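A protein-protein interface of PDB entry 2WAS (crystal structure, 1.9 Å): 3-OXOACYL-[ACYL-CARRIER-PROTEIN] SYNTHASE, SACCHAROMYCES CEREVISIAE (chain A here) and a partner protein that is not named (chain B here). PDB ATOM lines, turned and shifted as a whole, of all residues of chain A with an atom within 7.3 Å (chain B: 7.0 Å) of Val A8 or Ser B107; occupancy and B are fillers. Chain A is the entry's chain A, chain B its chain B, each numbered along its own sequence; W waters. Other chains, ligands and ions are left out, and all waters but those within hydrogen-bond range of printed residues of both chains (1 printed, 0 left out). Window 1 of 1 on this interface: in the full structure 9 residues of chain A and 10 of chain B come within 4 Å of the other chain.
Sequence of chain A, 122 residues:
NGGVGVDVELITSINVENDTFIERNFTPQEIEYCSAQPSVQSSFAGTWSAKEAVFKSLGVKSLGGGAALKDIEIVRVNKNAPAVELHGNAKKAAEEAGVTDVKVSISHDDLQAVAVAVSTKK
Among the printed residues, merely in contact across the chains: Gly A5 with Ser B105, Val A6 with Ile B106, Val A6 with Ser B107, Val A6 with Val B114, Asp A7 with Ser B107, Val A8 with His B108, Val A8 with Asp B109, Val A8 with Val B114, Leu A10 with Asp B109, Lys A56 with Ser B105 and Lys A56 with Ser B107.
Printed residues of chain B within 4 Å of Val A8: Ser B107 (3.0 Å), His B108 (3.4 Å), Asp B109 (3.5 Å) and Val B114 (3.96 Å).
Ser B107 touches just these residues of chain A: Val A6, Asp A7, Val A8 and Lys A56.
Of the printed residues of chain B, Asp A7 touches Ser B107 (3.5 Å).
Of the printed residues of chain A, Ile B106 touches Val A6 (3.7 Å) and Lys A56 (2.6 Å).
Printed residues of chain A within 4 Å of Ser B105: Gly A5, Val A6 and Lys A56.
The nearest printed residue of chain B that does not touch Val A8 is Gln B112 (4.4 Å).
The nearest residue of chain A that does not touch Ser B107 is Glu A9 (5.7 Å).
The backbone carbonyl oxygen (O) of Asp A7 lies within hydrogen-bond range of the backbone NH (N) of Ala A115 (2.9 Å).
NZ of Lys A56 sits at hydrogen-bond distance from O of Val A6, 2.8 Å away.
The side-chain carboxylate of Glu A9 sits close to the side-chain carboxylate of Asp A7, 2.4 Å away.
O of Leu A10 is in hydrogen-bond range of OG of Ser A13, at 3.1 Å.
The backbone NH (N) of Ser B105 sits at hydrogen-bond distance from the backbone carbonyl oxygen (O) of Val B116 (3.0 Å).
The backbone carbonyl oxygen of Ser B107 is in hydrogen-bond range of the backbone NH of Val B114, 2.8 Å away.
Hydrophobic or aromatic side chains of chain A within 4 Å of the printed part of chain B: Val A6, Val A8 and Leu A10.
Printed residues of chain B that touch a printed residue of chain A: Ser B105, Ile B106, Ser B107, His B108, Asp B109, Gln B112 and Val B114.
Among the printed residues, no Asp or Glu carboxylate lies within 4 Å of a Lys or Arg side-chain nitrogen of the other chain.
Water W1 lies within hydrogen-bond range of OG of Ser B107 (2.6 Å) and NZ of Lys A56 (3.0 Å).
OG of Ser B105 is in hydrogen-bond range of N of Val A6.
The backbone carbonyl oxygen of Ile B106 sits at hydrogen-bond distance from the side-chain amino group of Lys A56, at 2.6 Å.
The side-chain carboxylate of Asp B109 sits close to the side-chain amide oxygen of Gln A112 (3.3 Å).
OG of Ser B107 sits at hydrogen-bond distance from N of Val A8.
NE2 of Gln A112 sits close to NE2 of Gln B112 (2.9 Å).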
ATOM      1  N   GLY A   5     -18.102 -24.218 -20.989  1.00  0.00           N
ATOM      2  CA  GLY A   5     -17.354 -23.432 -20.031  1.00  0.00           C
ATOM      3  C   GLY A   5     -18.186 -22.294 -19.472  1.00  0.00           C
ATOM      4  O   GLY A   5     -18.972 -21.688 -20.177  1.00  0.00           O
ATOM      5  N   VAL A   6     -18.018 -22.003 -18.191  1.00  0.00           N
ATOM      6  CA  VAL A   6     -18.680 -20.863 -17.598  1.00  0.00           C
ATOM      7  C   VAL A   6     -17.658 -20.072 -16.788  1.00  0.00           C
ATOM      8  O   VAL A   6     -16.728 -20.638 -16.228  1.00  0.00           O
ATOM      9  CB  VAL A   6     -19.935 -21.269 -16.748  1.00  0.00           C
ATOM     10  CG1 VAL A   6     -19.544 -22.060 -15.536  1.00  0.00           C
ATOM     11  CG2 VAL A   6     -20.681 -20.044 -16.311  1.00  0.00           C
ATOM     12  N   ASP A   7     -17.803 -18.755 -16.773  1.00  0.00           N
ATOM     13  CA  ASP A   7     -16.943 -17.920 -15.954  1.00  0.00           C
ATOM     14  C   ASP A   7     -17.723 -16.718 -15.453  1.00  0.00           C
ATOM     15  O   ASP A   7     -18.461 -16.083 -16.200  1.00  0.00           O
ATOM     16  CB  ASP A   7     -15.682 -17.499 -16.728  1.00  0.00           C
ATOM     17  CG  ASP A   7     -14.605 -16.868 -15.833  1.00  0.00           C
ATOM     18  OD1 ASP A   7     -13.936 -17.608 -15.075  1.00  0.00           O
ATOM     19  OD2 ASP A   7     -14.388 -15.633 -15.915  1.00  0.00           O
ATOM     20  N   VAL A   8     -17.546 -16.427 -14.166  1.00  0.00           N
ATOM     21  CA  VAL A   8     -18.210 -15.321 -13.491  1.00  0.00           C
ATOM     22  C   VAL A   8     -17.104 -14.449 -12.889  1.00  0.00           C
ATOM     23  O   VAL A   8     -16.128 -14.968 -12.351  1.00  0.00           O
ATOM     24  CB  VAL A   8     -19.267 -15.845 -12.445  1.00  0.00           C
ATOM     25  CG1 VAL A   8     -18.590 -16.504 -11.282  1.00  0.00           C
ATOM     26  CG2 VAL A   8     -20.167 -14.737 -11.953  1.00  0.00           C
ATOM     27  N   GLU A   9     -17.221 -13.132 -13.065  1.00  0.00           N
ATOM     28  CA  GLU A   9     -16.255 -12.162 -12.543  1.00  0.00           C
ATOM     29  C   GLU A   9     -16.969 -10.995 -11.865  1.00  0.00           C
ATOM     30  O   GLU A   9     -18.041 -10.569 -12.297  1.00  0.00           O
ATOM     31  CB  GLU A   9     -15.390 -11.610 -13.670  1.00  0.00           C
ATOM     32  CG  GLU A   9     -14.789 -12.676 -14.525  1.00  0.00           C
ATOM     33  CD  GLU A   9     -13.551 -13.255 -13.892  1.00  0.00           C
ATOM     34  OE1 GLU A   9     -12.939 -12.512 -13.092  1.00  0.00           O
ATOM     35  OE2 GLU A   9     -13.174 -14.420 -14.185  1.00  0.00           O
ATOM     36  N   LEU A  10     -16.365 -10.483 -10.801  1.00  0.00           N
ATOM     37  CA  LEU A  10     -16.849  -9.261 -10.189  1.00  0.00           C
ATOM     38  C   LEU A  10     -16.463  -8.126 -11.149  1.00  0.00           C
ATOM     39  O   LEU A  10     -15.415  -8.168 -11.791  1.00  0.00           O
ATOM     40  CB  LEU A  10     -16.217  -9.071  -8.805  1.00  0.00           C
ATOM     41  CG  LEU A  10     -17.135  -8.579  -7.682  1.00  0.00           C
ATOM     42  CD1 LEU A  10     -18.150  -9.658  -7.273  1.00  0.00           C
ATOM     43  CD2 LEU A  10     -16.320  -8.117  -6.477  1.00  0.00           C
ATOM     44  N   SER A  13     -13.036  -6.594 -10.655  1.00  0.00           N
ATOM     45  CA  SER A  13     -11.814  -7.366 -10.889  1.00  0.00           C
ATOM     46  C   SER A  13     -11.004  -6.792 -12.064  1.00  0.00           C
ATOM     47  O   SER A  13      -9.827  -7.100 -12.243  1.00  0.00           O
ATOM     48  CB  SER A  13     -12.146  -8.835 -11.172  1.00  0.00           C
ATOM     49  OG  SER A  13     -12.499  -9.020 -12.543  1.00  0.00           O
ATOM     50  N   ALA A  45     -14.709  -6.702 -18.009  1.00  0.00           N
ATOM     51  CA  ALA A  45     -15.039  -7.822 -17.144  1.00  0.00           C
ATOM     52  C   ALA A  45     -15.809  -8.875 -17.924  1.00  0.00           C
ATOM     53  O   ALA A  45     -15.601 -10.079 -17.723  1.00  0.00           O
ATOM     54  CB  ALA A  45     -15.832  -7.345 -15.943  1.00  0.00           C
ATOM     55  N   TRP A  48     -13.350 -10.608 -20.418  1.00  0.00           N
ATOM     56  CA  TRP A  48     -12.502 -11.461 -19.608  1.00  0.00           C
ATOM     57  C   TRP A  48     -13.204 -12.778 -19.250  1.00  0.00           C
ATOM     58  O   TRP A  48     -12.604 -13.848 -19.334  1.00  0.00           O
ATOM     59  CB  TRP A  48     -12.073 -10.714 -18.339  1.00  0.00           C
ATOM     60  CG  TRP A  48     -11.202 -11.546 -17.451  1.00  0.00           C
ATOM     61  CD1 TRP A  48     -11.584 -12.216 -16.323  1.00  0.00           C
ATOM     62  CD2 TRP A  48      -9.817 -11.823 -17.627  1.00  0.00           C
ATOM     63  NE1 TRP A  48     -10.516 -12.897 -15.782  1.00  0.00           N
ATOM     64  CE2 TRP A  48      -9.398 -12.667 -16.576  1.00  0.00           C
ATOM     65  CE3 TRP A  48      -8.849 -11.439 -18.576  1.00  0.00           C
ATOM     66  CZ2 TRP A  48      -8.107 -13.131 -16.431  1.00  0.00           C
ATOM     67  CZ3 TRP A  48      -7.560 -11.899 -18.441  1.00  0.00           C
ATOM     68  CH2 TRP A  48      -7.198 -12.734 -17.380  1.00  0.00           C
ATOM     69  N   SER A  49     -14.470 -12.692 -18.841  1.00  0.00           N
ATOM     70  CA  SER A  49     -15.275 -13.879 -18.539  1.00  0.00           C
ATOM     71  C   SER A  49     -15.383 -14.763 -19.760  1.00  0.00           C
ATOM     72  O   SER A  49     -15.384 -15.996 -19.647  1.00  0.00           O
ATOM     73  CB  SER A  49     -16.689 -13.491 -18.127  1.00  0.00           C
ATOM     74  OG  SER A  49     -16.668 -12.623 -17.022  1.00  0.00           O
ATOM     75  N   GLU A  52     -12.109 -16.695 -20.346  1.00  0.00           N
ATOM     76  CA  GLU A  52     -12.050 -17.777 -19.375  1.00  0.00           C
ATOM     77  C   GLU A  52     -13.014 -18.909 -19.708  1.00  0.00           C
ATOM     78  O   GLU A  52     -12.647 -20.076 -19.663  1.00  0.00           O
ATOM     79  CB  GLU A  52     -12.349 -17.243 -17.982  1.00  0.00           C
ATOM     80  CG  GLU A  52     -11.278 -16.383 -17.419  1.00  0.00           C
ATOM     81  CD  GLU A  52     -10.110 -17.198 -16.900  1.00  0.00           C
ATOM     82  OE1 GLU A  52     -10.149 -18.444 -17.037  1.00  0.00           O
ATOM     83  OE2 GLU A  52      -9.152 -16.594 -16.354  1.00  0.00           O
ATOM     84  N   ALA A  53     -14.255 -18.550 -20.014  1.00  0.00           N
ATOM     85  CA  ALA A  53     -15.263 -19.530 -20.375  1.00  0.00           C
ATOM     86  C   ALA A  53     -14.816 -20.352 -21.569  1.00  0.00           C
ATOM     87  O   ALA A  53     -14.976 -21.566 -21.574  1.00  0.00           O
ATOM     88  CB  ALA A  53     -16.581 -18.851 -20.679  1.00  0.00           C
ATOM     89  N   LYS A  56     -12.046 -22.863 -20.868  1.00  0.00           N
ATOM     90  CA  LYS A  56     -12.667 -23.982 -20.138  1.00  0.00           C
ATOM     91  C   LYS A  56     -13.378 -24.992 -21.027  1.00  0.00           C
ATOM     92  O   LYS A  56     -13.330 -26.189 -20.777  1.00  0.00           O
ATOM     93  CB  LYS A  56     -13.670 -23.449 -19.117  1.00  0.00           C
ATOM     94  CG  LYS A  56     -13.065 -22.902 -17.859  1.00  0.00           C
ATOM     95  CD  LYS A  56     -14.125 -22.830 -16.766  1.00  0.00           C
ATOM     96  CE  LYS A  56     -13.690 -21.899 -15.658  1.00  0.00           C
ATOM     97  NZ  LYS A  56     -14.707 -21.774 -14.585  1.00  0.00           N
ATOM     98  N   LEU A 111     -23.435  -6.102 -10.540  1.00  0.00           N
ATOM     99  CA  LEU A 111     -22.616  -6.836  -9.591  1.00  0.00           C
ATOM    100  C   LEU A 111     -21.545  -7.683 -10.241  1.00  0.00           C
ATOM    101  O   LEU A 111     -20.454  -7.841  -9.703  1.00  0.00           O
ATOM    102  CB  LEU A 111     -23.501  -7.771  -8.797  1.00  0.00           C
ATOM    103  CG  LEU A 111     -24.326  -7.095  -7.725  1.00  0.00           C
ATOM    104  CD1 LEU A 111     -25.444  -8.004  -7.250  1.00  0.00           C
ATOM    105  CD2 LEU A 111     -23.404  -6.738  -6.596  1.00  0.00           C
ATOM    106  N   GLN A 112     -21.854  -8.246 -11.397  1.00  0.00           N
ATOM    107  CA  GLN A 112     -20.946  -9.215 -11.967  1.00  0.00           C
ATOM    108  C   GLN A 112     -21.188  -9.476 -13.444  1.00  0.00           C
ATOM    109  O   GLN A 112     -22.218  -9.100 -14.016  1.00  0.00           O
ATOM    110  CB  GLN A 112     -21.056 -10.499 -11.160  1.00  0.00           C
ATOM    111  CG  GLN A 112     -22.367 -11.266 -11.396  1.00  0.00           C
ATOM    112  CD  GLN A 112     -22.553 -12.396 -10.416  1.00  0.00           C
ATOM    113  OE1 GLN A 112     -22.480 -12.192  -9.202  1.00  0.00           O
ATOM    114  NE2 GLN A 112     -22.800 -13.588 -10.928  1.00  0.00           N
ATOM    115  N   ALA A 113     -20.217 -10.116 -14.065  1.00  0.00           N
ATOM    116  CA  ALA A 113     -20.379 -10.541 -15.443  1.00  0.00           C
ATOM    117  C   ALA A 113     -20.369 -12.052 -15.482  1.00  0.00           C
ATOM    118  O   ALA A 113     -19.742 -12.689 -14.642  1.00  0.00           O
ATOM    119  CB  ALA A 113     -19.258  -9.993 -16.316  1.00  0.00           C
ATOM    120  N   VAL A 114     -21.072 -12.628 -16.457  1.00  0.00           N
ATOM    121  CA  VAL A 114     -21.098 -14.074 -16.647  1.00  0.00           C
ATOM    122  C   VAL A 114     -20.880 -14.353 -18.120  1.00  0.00           C
ATOM    123  O   VAL A 114     -21.365 -13.610 -18.973  1.00  0.00           O
ATOM    124  CB  VAL A 114     -22.462 -14.705 -16.227  1.00  0.00           C
ATOM    125  CG1 VAL A 114     -22.393 -16.217 -16.299  1.00  0.00           C
ATOM    126  CG2 VAL A 114     -22.841 -14.283 -14.834  1.00  0.00           C
ATOM    127  N   ALA A 115     -20.151 -15.418 -18.422  1.00  0.00           N
ATOM    128  CA  ALA A 115     -20.023 -15.878 -19.796  1.00  0.00           C
ATOM    129  C   ALA A 115     -20.156 -17.389 -19.850  1.00  0.00           C
ATOM    130  O   ALA A 115     -19.696 -18.084 -18.958  1.00  0.00           O
ATOM    131  CB  ALA A 115     -18.704 -15.409 -20.431  1.00  0.00           C
ATOM    132  N   ASP B   7     -27.313 -23.512 -12.469  1.00  0.00           N
ATOM    133  CA  ASP B   7     -27.565 -23.324 -11.044  1.00  0.00           C
ATOM    134  C   ASP B   7     -26.627 -22.266 -10.455  1.00  0.00           C
ATOM    135  O   ASP B   7     -25.435 -22.251 -10.714  1.00  0.00           O
ATOM    136  CB  ASP B   7     -27.469 -24.647 -10.276  1.00  0.00           C
ATOM    137  CG  ASP B   7     -28.042 -24.553  -8.877  1.00  0.00           C
ATOM    138  OD1 ASP B   7     -29.272 -24.519  -8.733  1.00  0.00           O
ATOM    139  OD2 ASP B   7     -27.269 -24.522  -7.913  1.00  0.00           O
ATOM    140  N   ILE B  11     -22.563 -18.083  -1.761  1.00  0.00           N
ATOM    141  CA  ILE B  11     -21.451 -18.833  -1.186  1.00  0.00           C
ATOM    142  C   ILE B  11     -21.789 -19.314   0.215  1.00  0.00           C
ATOM    143  O   ILE B  11     -21.409 -20.395   0.630  1.00  0.00           O
ATOM    144  CB  ILE B  11     -20.172 -18.005  -1.143  1.00  0.00           C
ATOM    145  CG1 ILE B  11     -19.833 -17.484  -2.543  1.00  0.00           C
ATOM    146  CG2 ILE B  11     -19.026 -18.812  -0.543  1.00  0.00           C
ATOM    147  CD1 ILE B  11     -19.208 -18.475  -3.443  1.00  0.00           C
ATOM    148  N   SER B  42     -16.386 -21.736  -0.916  1.00  0.00           N
ATOM    149  CA  SER B  42     -16.644 -21.416  -2.317  1.00  0.00           C
ATOM    150  C   SER B  42     -16.584 -22.674  -3.130  1.00  0.00           C
ATOM    151  O   SER B  42     -17.370 -22.862  -4.047  1.00  0.00           O
ATOM    152  CB  SER B  42     -15.597 -20.456  -2.876  1.00  0.00           C
ATOM    153  OG  SER B  42     -15.719 -19.191  -2.298  1.00  0.00           O
ATOM    154  N   ALA B  45     -19.741 -24.768  -2.602  1.00  0.00           N
ATOM    155  CA  ALA B  45     -20.824 -24.036  -3.256  1.00  0.00           C
ATOM    156  C   ALA B  45     -20.825 -24.245  -4.757  1.00  0.00           C
ATOM    157  O   ALA B  45     -21.877 -24.377  -5.365  1.00  0.00           O
ATOM    158  CB  ALA B  45     -20.747 -22.539  -2.932  1.00  0.00           C
ATOM    159  N   GLY B  46     -19.636 -24.284  -5.342  1.00  0.00           N
ATOM    160  CA  GLY B  46     -19.462 -24.543  -6.758  1.00  0.00           C
ATOM    161  C   GLY B  46     -19.818 -25.955  -7.162  1.00  0.00           C
ATOM    162  O   GLY B  46     -20.504 -26.153  -8.149  1.00  0.00           O
ATOM    163  N   SER B  49     -23.568 -26.365  -6.955  1.00  0.00           N
ATOM    164  CA  SER B  49     -24.211 -25.793  -8.145  1.00  0.00           C
ATOM    165  C   SER B  49     -24.126 -26.749  -9.326  1.00  0.00           C
ATOM    166  O   SER B  49     -25.067 -26.866 -10.098  1.00  0.00           O
ATOM    167  CB  SER B  49     -23.539 -24.479  -8.536  1.00  0.00           C
ATOM    168  OG  SER B  49     -23.555 -23.582  -7.457  1.00  0.00           O
ATOM    169  N   ARG B  76     -13.144 -33.703 -10.345  1.00  0.00           N
ATOM    170  CA  ARG B  76     -12.224 -32.651 -10.736  1.00  0.00           C
ATOM    171  C   ARG B  76     -10.884 -33.193 -10.311  1.00  0.00           C
ATOM    172  O   ARG B  76     -10.533 -33.097  -9.138  1.00  0.00           O
ATOM    173  CB  ARG B  76     -12.546 -31.376  -9.949  1.00  0.00           C
ATOM    174  CG  ARG B  76     -14.055 -31.074  -9.864  1.00  0.00           C
ATOM    175  CD  ARG B  76     -14.465 -30.128  -8.734  1.00  0.00           C
ATOM    176  NE  ARG B  76     -14.489 -28.745  -9.216  1.00  0.00           N
ATOM    177  CZ  ARG B  76     -14.976 -27.696  -8.547  1.00  0.00           C
ATOM    178  NH1 ARG B  76     -15.502 -27.850  -7.337  1.00  0.00           N
ATOM    179  NH2 ARG B  76     -14.938 -26.480  -9.098  1.00  0.00           N
ATOM    180  N   SER B 105     -19.536 -27.170 -16.279  1.00  0.00           N
ATOM    181  CA  SER B 105     -18.511 -26.200 -15.934  1.00  0.00           C
ATOM    182  C   SER B 105     -18.967 -25.397 -14.702  1.00  0.00           C
ATOM    183  O   SER B 105     -20.161 -25.199 -14.497  1.00  0.00           O
ATOM    184  CB  SER B 105     -18.207 -25.301 -17.124  1.00  0.00           C
ATOM    185  OG  SER B 105     -17.064 -24.501 -16.876  1.00  0.00           O
ATOM    186  N   ILE B 106     -18.007 -24.964 -13.885  1.00  0.00           N
ATOM    187  CA  ILE B 106     -18.283 -24.312 -12.619  1.00  0.00           C
ATOM    188  C   ILE B 106     -17.483 -23.028 -12.491  1.00  0.00           C
ATOM    189  O   ILE B 106     -16.333 -22.960 -12.938  1.00  0.00           O
ATOM    190  CB  ILE B 106     -17.870 -25.217 -11.451  1.00  0.00           C
ATOM    191  CG1 ILE B 106     -18.535 -26.588 -11.574  1.00  0.00           C
ATOM    192  CG2 ILE B 106     -18.240 -24.594 -10.131  1.00  0.00           C
ATOM    193  CD1 ILE B 106     -17.957 -27.637 -10.649  1.00  0.00           C
ATOM    194  N   SER B 107     -18.081 -22.007 -11.883  1.00  0.00           N
ATOM    195  CA  SER B 107     -17.357 -20.768 -11.582  1.00  0.00           C
ATOM    196  C   SER B 107     -17.924 -20.084 -10.336  1.00  0.00           C
ATOM    197  O   SER B 107     -19.052 -20.315  -9.958  1.00  0.00           O
ATOM    198  CB  SER B 107     -17.386 -19.828 -12.791  1.00  0.00           C
ATOM    199  OG  SER B 107     -16.457 -18.776 -12.631  1.00  0.00           O
ATOM    200  N   HIS B 108     -17.123 -19.260  -9.686  1.00  0.00           N
ATOM    201  CA  HIS B 108     -17.634 -18.446  -8.601  1.00  0.00           C
ATOM    202  C   HIS B 108     -16.844 -17.152  -8.486  1.00  0.00           C
ATOM    203  O   HIS B 108     -15.758 -17.029  -9.038  1.00  0.00           O
ATOM    204  CB  HIS B 108     -17.606 -19.208  -7.264  1.00  0.00           C
ATOM    205  CG  HIS B 108     -16.228 -19.526  -6.777  1.00  0.00           C
ATOM    206  ND1 HIS B 108     -15.481 -18.647  -6.024  1.00  0.00           N
ATOM    207  CD2 HIS B 108     -15.449 -20.615  -6.968  1.00  0.00           C
ATOM    208  CE1 HIS B 108     -14.300 -19.174  -5.774  1.00  0.00           C
ATOM    209  NE2 HIS B 108     -14.254 -20.375  -6.332  1.00  0.00           N
ATOM    210  N   ASP B 109     -17.429 -16.187  -7.793  1.00  0.00           N
ATOM    211  CA  ASP B 109     -16.719 -14.981  -7.381  1.00  0.00           C
ATOM    212  C   ASP B 109     -16.999 -14.821  -5.881  1.00  0.00           C
ATOM    213  O   ASP B 109     -17.395 -15.802  -5.226  1.00  0.00           O
ATOM    214  CB  ASP B 109     -17.182 -13.737  -8.173  1.00  0.00           C
ATOM    215  CG  ASP B 109     -18.695 -13.538  -8.161  1.00  0.00           C
ATOM    216  OD1 ASP B 109     -19.346 -13.976  -7.208  1.00  0.00           O
ATOM    217  OD2 ASP B 109     -19.235 -12.913  -9.103  1.00  0.00           O
ATOM    218  N   ASP B 110     -16.824 -13.615  -5.337  1.00  0.00           N
ATOM    219  CA  ASP B 110     -17.110 -13.355  -3.924  1.00  0.00           C
ATOM    220  C   ASP B 110     -18.551 -13.544  -3.512  1.00  0.00           C
ATOM    221  O   ASP B 110     -18.835 -13.856  -2.370  1.00  0.00           O
ATOM    222  CB  ASP B 110     -16.686 -11.931  -3.590  1.00  0.00           C
ATOM    223  CG  ASP B 110     -15.217 -11.812  -3.388  1.00  0.00           C
ATOM    224  OD1 ASP B 110     -14.601 -12.859  -3.175  1.00  0.00           O
ATOM    225  OD2 ASP B 110     -14.684 -10.685  -3.499  1.00  0.00           O
ATOM    226  N   GLN B 112     -21.188 -15.427  -5.335  1.00  0.00           N
ATOM    227  CA  GLN B 112     -21.977 -16.576  -5.717  1.00  0.00           C
ATOM    228  C   GLN B 112     -21.234 -17.521  -6.634  1.00  0.00           C
ATOM    229  O   GLN B 112     -20.194 -17.193  -7.213  1.00  0.00           O
ATOM    230  CB  GLN B 112     -23.282 -16.107  -6.371  1.00  0.00           C
ATOM    231  CG  GLN B 112     -23.074 -15.568  -7.782  1.00  0.00           C
ATOM    232  CD  GLN B 112     -24.289 -14.815  -8.297  1.00  0.00           C
ATOM    233  OE1 GLN B 112     -24.812 -13.915  -7.616  1.00  0.00           O
ATOM    234  NE2 GLN B 112     -24.740 -15.166  -9.511  1.00  0.00           N
ATOM    235  N   ALA B 113     -21.795 -18.720  -6.740  1.00  0.00           N
ATOM    236  CA  ALA B 113     -21.270 -19.738  -7.626  1.00  0.00           C
ATOM    237  C   ALA B 113     -22.298 -20.017  -8.712  1.00  0.00           C
ATOM    238  O   ALA B 113     -23.512 -19.933  -8.476  1.00  0.00           O
ATOM    239  CB  ALA B 113     -20.952 -21.007  -6.855  1.00  0.00           C
ATOM    240  N   VAL B 114     -21.811 -20.332  -9.903  1.00  0.00           N
ATOM    241  CA  VAL B 114     -22.672 -20.675 -11.018  1.00  0.00           C
ATOM    242  C   VAL B 114     -22.151 -21.946 -11.654  1.00  0.00           C
ATOM    243  O   VAL B 114     -20.958 -22.178 -11.709  1.00  0.00           O
ATOM    244  CB  VAL B 114     -22.734 -19.539 -12.072  1.00  0.00           C
ATOM    245  CG1 VAL B 114     -23.382 -18.312 -11.479  1.00  0.00           C
ATOM    246  CG2 VAL B 114     -21.333 -19.217 -12.586  1.00  0.00           C
ATOM    247  N   ALA B 115     -23.061 -22.794 -12.108  1.00  0.00           N
ATOM    248  CA  ALA B 115     -22.672 -23.954 -12.845  1.00  0.00           C
ATOM    249  C   ALA B 115     -23.617 -24.124 -14.019  1.00  0.00           C
ATOM    250  O   ALA B 115     -24.797 -23.836 -13.922  1.00  0.00           O
ATOM    251  CB  ALA B 115     -22.672 -25.164 -11.946  1.00  0.00           C
ATOM    252  N   VAL B 116     -23.065 -24.544 -15.148  1.00  0.00           N
ATOM    253  CA  VAL B 116     -23.858 -24.848 -16.341  1.00  0.00           C
ATOM    254  C   VAL B 116     -23.542 -26.263 -16.822  1.00  0.00           C
ATOM    255  O   VAL B 116     -22.381 -26.636 -16.908  1.00  0.00           O
ATOM    256  CB  VAL B 116     -23.623 -23.810 -17.486  1.00  0.00           C
ATOM    257  CG1 VAL B 116     -24.435 -24.159 -18.732  1.00  0.00           C
ATOM    258  CG2 VAL B 116     -23.968 -22.405 -17.001  1.00  0.00           C
HETATM  259  O   HOH W   1     -14.162 -19.908 -12.304  1.00  0.00           O
